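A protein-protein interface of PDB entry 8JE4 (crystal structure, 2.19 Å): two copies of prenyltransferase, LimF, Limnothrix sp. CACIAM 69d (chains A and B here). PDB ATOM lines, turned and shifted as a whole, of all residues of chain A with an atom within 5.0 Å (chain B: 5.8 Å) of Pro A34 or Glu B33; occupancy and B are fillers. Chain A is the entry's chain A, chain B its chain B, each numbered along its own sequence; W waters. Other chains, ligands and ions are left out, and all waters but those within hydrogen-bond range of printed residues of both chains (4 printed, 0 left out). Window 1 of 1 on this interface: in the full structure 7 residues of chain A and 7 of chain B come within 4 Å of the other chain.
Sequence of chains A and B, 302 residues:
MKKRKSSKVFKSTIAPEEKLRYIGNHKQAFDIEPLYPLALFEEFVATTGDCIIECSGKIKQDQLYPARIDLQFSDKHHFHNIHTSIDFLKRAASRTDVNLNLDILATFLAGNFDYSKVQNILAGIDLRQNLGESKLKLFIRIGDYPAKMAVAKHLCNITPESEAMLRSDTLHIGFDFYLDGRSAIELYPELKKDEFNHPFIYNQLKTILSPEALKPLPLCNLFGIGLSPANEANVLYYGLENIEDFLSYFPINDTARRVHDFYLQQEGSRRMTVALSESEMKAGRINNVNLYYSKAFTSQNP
Pro A34 touches Glu B33, but with the chains exchanged Glu A33 does not touch Pro B34 (6.4 Å). Pro A34 touches its own counterpart, Pro B34. Leu A35 touches Glu B33, but with the chains exchanged Glu A33 does not touch Leu B35 (5.2 Å). Tyr A36 touches Glu B33, but with the chains exchanged Glu A33 does not touch Tyr B36 (4.7 Å). Positions printed for both chains: 32, 33, 34, 35, 36 and 38. Of the 7 pairs that touch across the chains among the printed residues, 1 has its exchanged pair printed and touching as well.
Water W1 lies within hydrogen-bond range of O of Pro A34 and NE2 of Gln B129. Water W2 lies within hydrogen-bond range of the side-chain carboxylate (OE1) of Glu A33 and the backbone NH (N) of Tyr B36. Water W4 lies within hydrogen-bond range of OE2 of Glu B33 (2.6 Å), O of Asp B31 (2.9 Å) and NH1 of Arg A95 (3.3 Å). Water W3 bridges the backbone NH (N) of Tyr A36 and the side-chain amide nitrogen (NE2) of Gln B129.
The backbone NH (N) of Tyr A36 lies within hydrogen-bond range of the side-chain carboxylate (OE1) of Glu B33, at 3.5 Å. The guanidinium group (NE) of Arg A95 is in salt-bridge range of the side-chain carboxylate (OD2) of Asp B31, 3.6 Å away.
CG of Glu A33 touches O of Gln B129, at 3.6 Å. Pro A34 touches Glu B33 (O to CB, 3.9 Å). Pro A34 touches Pro B34. C of Leu A35 touches OE1 of Glu B33 (3.5 Å). CD2 of Leu A35 touches NE2 of Gln B129, at 3.7 Å.
Of the printed residues of chain B, Pro A34 touches Glu B33 and Pro B34. Glu B33 touches just these residues of chain A: Pro A34, Leu A35 and Tyr A36. Of the printed residues of chain B, Glu A33 touches Gln B129. Printed residues of chain B within 4 Å of Arg A95: Asp B31. Of the printed residues of chain B, Tyr A36 touches Glu B33 (3.2 Å). Of the printed residues of chain A, Gln B129 touches Glu A33 (3.6 Å) and Leu A35 (3.7 Å). The nearest residue of chain B that does not touch Pro A34 is Leu B35 (4.1 Å). The nearest residue of chain A that does not touch Glu B33 is Arg A95 (4.4 Å). The nearest printed residue of chain B that does not touch Leu A35 is Leu B35 (6.2 Å).
Printed residues of chain B that touch a printed residue of chain A: Asp B31, Glu B33, Pro B34 and Gln B129. Of the 8 printed residues of chain A, 5 touch a printed residue of chain B. Hydrophobic or aromatic side chains of chain A within 4 Å of the printed part of chain B: Pro A34, Leu A35 and Tyr A36. Among the printed residues, 7 pairs touch across the chains.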
ATOM      1  N   ILE A  32       7.954  -5.609 -28.246  1.00  0.00           N
ATOM      2  CA  ILE A  32       7.349  -6.935 -28.309  1.00  0.00           C
ATOM      3  C   ILE A  32       8.374  -7.901 -28.892  1.00  0.00           C
ATOM      4  O   ILE A  32       8.658  -7.871 -30.091  1.00  0.00           O
ATOM      5  CB  ILE A  32       6.058  -6.930 -29.135  1.00  0.00           C
ATOM      6  CG1 ILE A  32       5.058  -5.914 -28.577  1.00  0.00           C
ATOM      7  CG2 ILE A  32       5.435  -8.313 -29.142  1.00  0.00           C
ATOM      8  CD1 ILE A  32       3.734  -5.906 -29.305  1.00  0.00           C
ATOM      9  N   GLU A  33       8.932  -8.753 -28.044  1.00  0.00           N
ATOM     10  CA  GLU A  33       9.831  -9.805 -28.489  1.00  0.00           C
ATOM     11  C   GLU A  33       9.012 -11.015 -28.924  1.00  0.00           C
ATOM     12  O   GLU A  33       7.818 -11.104 -28.634  1.00  0.00           O
ATOM     13  CB  GLU A  33      10.814 -10.144 -27.371  1.00  0.00           C
ATOM     14  CG  GLU A  33      11.673  -8.959 -26.918  1.00  0.00           C
ATOM     15  CD  GLU A  33      12.421  -8.294 -28.065  1.00  0.00           C
ATOM     16  OE1 GLU A  33      12.861  -9.007 -28.992  1.00  0.00           O
ATOM     17  OE2 GLU A  33      12.575  -7.056 -28.038  1.00  0.00           O
ATOM     18  N   PRO A  34       9.617 -11.952 -29.656  1.00  0.00           N
ATOM     19  CA  PRO A  34       8.850 -13.105 -30.159  1.00  0.00           C
ATOM     20  C   PRO A  34       8.179 -13.893 -29.044  1.00  0.00           C
ATOM     21  O   PRO A  34       8.834 -14.428 -28.147  1.00  0.00           O
ATOM     22  CB  PRO A  34       9.909 -13.939 -30.883  1.00  0.00           C
ATOM     23  CG  PRO A  34      10.901 -12.947 -31.339  1.00  0.00           C
ATOM     24  CD  PRO A  34      10.965 -11.902 -30.252  1.00  0.00           C
ATOM     25  N   LEU A  35       6.852 -13.948 -29.106  1.00  0.00           N
ATOM     26  CA  LEU A  35       6.040 -14.782 -28.234  1.00  0.00           C
ATOM     27  C   LEU A  35       5.231 -15.736 -29.099  1.00  0.00           C
ATOM     28  O   LEU A  35       4.704 -15.341 -30.142  1.00  0.00           O
ATOM     29  CB  LEU A  35       5.100 -13.941 -27.366  1.00  0.00           C
ATOM     30  CG  LEU A  35       5.711 -13.008 -26.320  1.00  0.00           C
ATOM     31  CD1 LEU A  35       4.618 -12.160 -25.692  1.00  0.00           C
ATOM     32  CD2 LEU A  35       6.460 -13.806 -25.261  1.00  0.00           C
ATOM     33  N   TYR A  36       5.136 -16.989 -28.678  1.00  0.00           N
ATOM     34  CA  TYR A  36       4.387 -17.960 -29.462  1.00  0.00           C
ATOM     35  C   TYR A  36       2.893 -17.651 -29.386  1.00  0.00           C
ATOM     36  O   TYR A  36       2.374 -17.355 -28.306  1.00  0.00           O
ATOM     37  CB  TYR A  36       4.658 -19.381 -28.960  1.00  0.00           C
ATOM     38  CG  TYR A  36       4.005 -20.461 -29.796  1.00  0.00           C
ATOM     39  CD1 TYR A  36       4.613 -20.938 -30.947  1.00  0.00           C
ATOM     40  CD2 TYR A  36       2.781 -21.005 -29.433  1.00  0.00           C
ATOM     41  CE1 TYR A  36       4.021 -21.922 -31.714  1.00  0.00           C
ATOM     42  CE2 TYR A  36       2.179 -21.989 -30.195  1.00  0.00           C
ATOM     43  CZ  TYR A  36       2.806 -22.443 -31.336  1.00  0.00           C
ATOM     44  OH  TYR A  36       2.219 -23.426 -32.102  1.00  0.00           O
ATOM     45  N   LEU A  38       3.423 -15.699 -32.390  1.00  0.00           N
ATOM     46  CA  LEU A  38       3.396 -14.448 -33.146  1.00  0.00           C
ATOM     47  C   LEU A  38       3.881 -14.648 -34.577  1.00  0.00           C
ATOM     48  O   LEU A  38       3.283 -14.119 -35.521  1.00  0.00           O
ATOM     49  CB  LEU A  38       4.247 -13.388 -32.444  1.00  0.00           C
ATOM     50  CG  LEU A  38       4.338 -12.008 -33.095  1.00  0.00           C
ATOM     51  CD1 LEU A  38       2.961 -11.364 -33.155  1.00  0.00           C
ATOM     52  CD2 LEU A  38       5.314 -11.126 -32.331  1.00  0.00           C
ATOM     53  N   ALA A  39       4.967 -15.403 -34.754  1.00  0.00           N
ATOM     54  CA  ALA A  39       5.486 -15.659 -36.093  1.00  0.00           C
ATOM     55  C   ALA A  39       4.443 -16.353 -36.961  1.00  0.00           C
ATOM     56  O   ALA A  39       4.255 -15.996 -38.129  1.00  0.00           O
ATOM     57  CB  ALA A  39       6.764 -16.495 -36.009  1.00  0.00           C
ATOM     58  N   ARG A  95       1.843 -27.298 -31.247  1.00  0.00           N
ATOM     59  CA  ARG A  95       2.878 -27.349 -30.222  1.00  0.00           C
ATOM     60  C   ARG A  95       2.463 -28.304 -29.106  1.00  0.00           C
ATOM     61  O   ARG A  95       1.314 -28.296 -28.657  1.00  0.00           O
ATOM     62  CB  ARG A  95       3.144 -25.950 -29.663  1.00  0.00           C
ATOM     63  CG  ARG A  95       4.288 -25.889 -28.666  1.00  0.00           C
ATOM     64  CD  ARG A  95       4.653 -24.452 -28.326  1.00  0.00           C
ATOM     65  NE  ARG A  95       5.368 -24.354 -27.059  1.00  0.00           N
ATOM     66  CZ  ARG A  95       6.032 -23.280 -26.654  1.00  0.00           C
ATOM     67  NH1 ARG A  95       6.125 -22.199 -27.412  1.00  0.00           N
ATOM     68  NH2 ARG A  95       6.626 -23.295 -25.464  1.00  0.00           N
ATOM     69  N   ASP B  31      10.928 -25.819 -28.436  1.00  0.00           N
ATOM     70  CA  ASP B  31       9.967 -24.788 -28.838  1.00  0.00           C
ATOM     71  C   ASP B  31      10.557 -23.385 -28.700  1.00  0.00           C
ATOM     72  O   ASP B  31       9.945 -22.479 -28.131  1.00  0.00           O
ATOM     73  CB  ASP B  31       8.673 -24.919 -28.033  1.00  0.00           C
ATOM     74  CG  ASP B  31       8.048 -26.296 -28.153  1.00  0.00           C
ATOM     75  OD1 ASP B  31       7.786 -26.729 -29.294  1.00  0.00           O
ATOM     76  OD2 ASP B  31       7.828 -26.950 -27.111  1.00  0.00           O
ATOM     77  N   ILE B  32      11.757 -23.205 -29.240  1.00  0.00           N
ATOM     78  CA  ILE B  32      12.479 -21.947 -29.092  1.00  0.00           C
ATOM     79  C   ILE B  32      11.956 -20.946 -30.115  1.00  0.00           C
ATOM     80  O   ILE B  32      11.931 -21.224 -31.318  1.00  0.00           O
ATOM     81  CB  ILE B  32      13.991 -22.158 -29.245  1.00  0.00           C
ATOM     82  CG1 ILE B  32      14.490 -23.204 -28.242  1.00  0.00           C
ATOM     83  CG2 ILE B  32      14.734 -20.848 -29.041  1.00  0.00           C
ATOM     84  CD1 ILE B  32      15.983 -23.453 -28.309  1.00  0.00           C
ATOM     85  N   GLU B  33      11.534 -19.777 -29.633  1.00  0.00           N
ATOM     86  CA  GLU B  33      11.078 -18.709 -30.506  1.00  0.00           C
ATOM     87  C   GLU B  33      12.268 -18.028 -31.180  1.00  0.00           C
ATOM     88  O   GLU B  33      13.407 -18.157 -30.724  1.00  0.00           O
ATOM     89  CB  GLU B  33      10.269 -17.690 -29.706  1.00  0.00           C
ATOM     90  CG  GLU B  33       8.911 -18.204 -29.254  1.00  0.00           C
ATOM     91  CD  GLU B  33       7.931 -18.357 -30.403  1.00  0.00           C
ATOM     92  OE1 GLU B  33       7.642 -17.349 -31.083  1.00  0.00           O
ATOM     93  OE2 GLU B  33       7.453 -19.488 -30.632  1.00  0.00           O
ATOM     94  N   PRO B  34      12.032 -17.295 -32.277  1.00  0.00           N
ATOM     95  CA  PRO B  34      13.143 -16.584 -32.929  1.00  0.00           C
ATOM     96  C   PRO B  34      13.637 -15.397 -32.114  1.00  0.00           C
ATOM     97  O   PRO B  34      13.552 -14.247 -32.559  1.00  0.00           O
ATOM     98  CB  PRO B  34      12.540 -16.130 -34.267  1.00  0.00           C
ATOM     99  CG  PRO B  34      11.321 -16.980 -34.458  1.00  0.00           C
ATOM    100  CD  PRO B  34      10.800 -17.232 -33.082  1.00  0.00           C
ATOM    101  N   LEU B  35      14.170 -15.667 -30.924  1.00  0.00           N
ATOM    102  CA  LEU B  35      14.677 -14.601 -30.073  1.00  0.00           C
ATOM    103  C   LEU B  35      15.876 -13.919 -30.725  1.00  0.00           C
ATOM    104  O   LEU B  35      16.636 -14.532 -31.479  1.00  0.00           O
ATOM    105  CB  LEU B  35      15.066 -15.159 -28.702  1.00  0.00           C
ATOM    106  CG  LEU B  35      13.973 -15.876 -27.901  1.00  0.00           C
ATOM    107  CD1 LEU B  35      14.542 -16.481 -26.619  1.00  0.00           C
ATOM    108  CD2 LEU B  35      12.823 -14.930 -27.595  1.00  0.00           C
ATOM    109  N   TYR B  36      16.033 -12.635 -30.437  1.00  0.00           N
ATOM    110  CA  TYR B  36      17.143 -11.883 -31.001  1.00  0.00           C
ATOM    111  C   TYR B  36      18.410 -12.124 -30.180  1.00  0.00           C
ATOM    112  O   TYR B  36      18.355 -12.136 -28.948  1.00  0.00           O
ATOM    113  CB  TYR B  36      16.817 -10.390 -31.029  1.00  0.00           C
ATOM    114  CG  TYR B  36      17.862  -9.536 -31.707  1.00  0.00           C
ATOM    115  CD1 TYR B  36      17.864  -9.373 -33.085  1.00  0.00           C
ATOM    116  CD2 TYR B  36      18.837  -8.881 -30.968  1.00  0.00           C
ATOM    117  CE1 TYR B  36      18.815  -8.588 -33.711  1.00  0.00           C
ATOM    118  CE2 TYR B  36      19.792  -8.095 -31.584  1.00  0.00           C
ATOM    119  CZ  TYR B  36      19.777  -7.952 -32.956  1.00  0.00           C
ATOM    120  OH  TYR B  36      20.727  -7.168 -33.571  1.00  0.00           O
ATOM    121  N   LEU B  38      19.126 -14.795 -32.539  1.00  0.00           N
ATOM    122  CA  LEU B  38      19.390 -16.190 -32.887  1.00  0.00           C
ATOM    123  C   LEU B  38      19.649 -16.354 -34.379  1.00  0.00           C
ATOM    124  O   LEU B  38      20.525 -17.128 -34.783  1.00  0.00           O
ATOM    125  CB  LEU B  38      18.222 -17.075 -32.448  1.00  0.00           C
ATOM    126  CG  LEU B  38      18.299 -18.563 -32.794  1.00  0.00           C
ATOM    127  CD1 LEU B  38      19.459 -19.237 -32.073  1.00  0.00           C
ATOM    128  CD2 LEU B  38      16.986 -19.254 -32.467  1.00  0.00           C
ATOM    129  N   GLN B 129      13.391 -14.215 -22.890  1.00  0.00           N
ATOM    130  CA  GLN B 129      12.229 -13.502 -23.411  1.00  0.00           C
ATOM    131  C   GLN B 129      12.381 -11.996 -23.226  1.00  0.00           C
ATOM    132  O   GLN B 129      11.959 -11.216 -24.089  1.00  0.00           O
ATOM    133  CB  GLN B 129      10.951 -14.005 -22.739  1.00  0.00           C
ATOM    134  CG  GLN B 129      10.345 -15.240 -23.390  1.00  0.00           C
ATOM    135  CD  GLN B 129       8.989 -15.603 -22.809  1.00  0.00           C
ATOM    136  OE1 GLN B 129       8.608 -15.115 -21.744  1.00  0.00           O
ATOM    137  NE2 GLN B 129       8.256 -16.463 -23.506  1.00  0.00           N
HETATM  138  O   HOH W   1       8.831 -16.151 -26.404  1.00  0.00           O
HETATM  139  O   HOH W   2      14.060 -11.272 -29.144  1.00  0.00           O
HETATM  140  O   HOH W   3       6.630 -17.670 -26.276  1.00  0.00           O
HETATM  141  O   HOH W   4       7.954 -21.983 -30.127  1.00  0.00           O
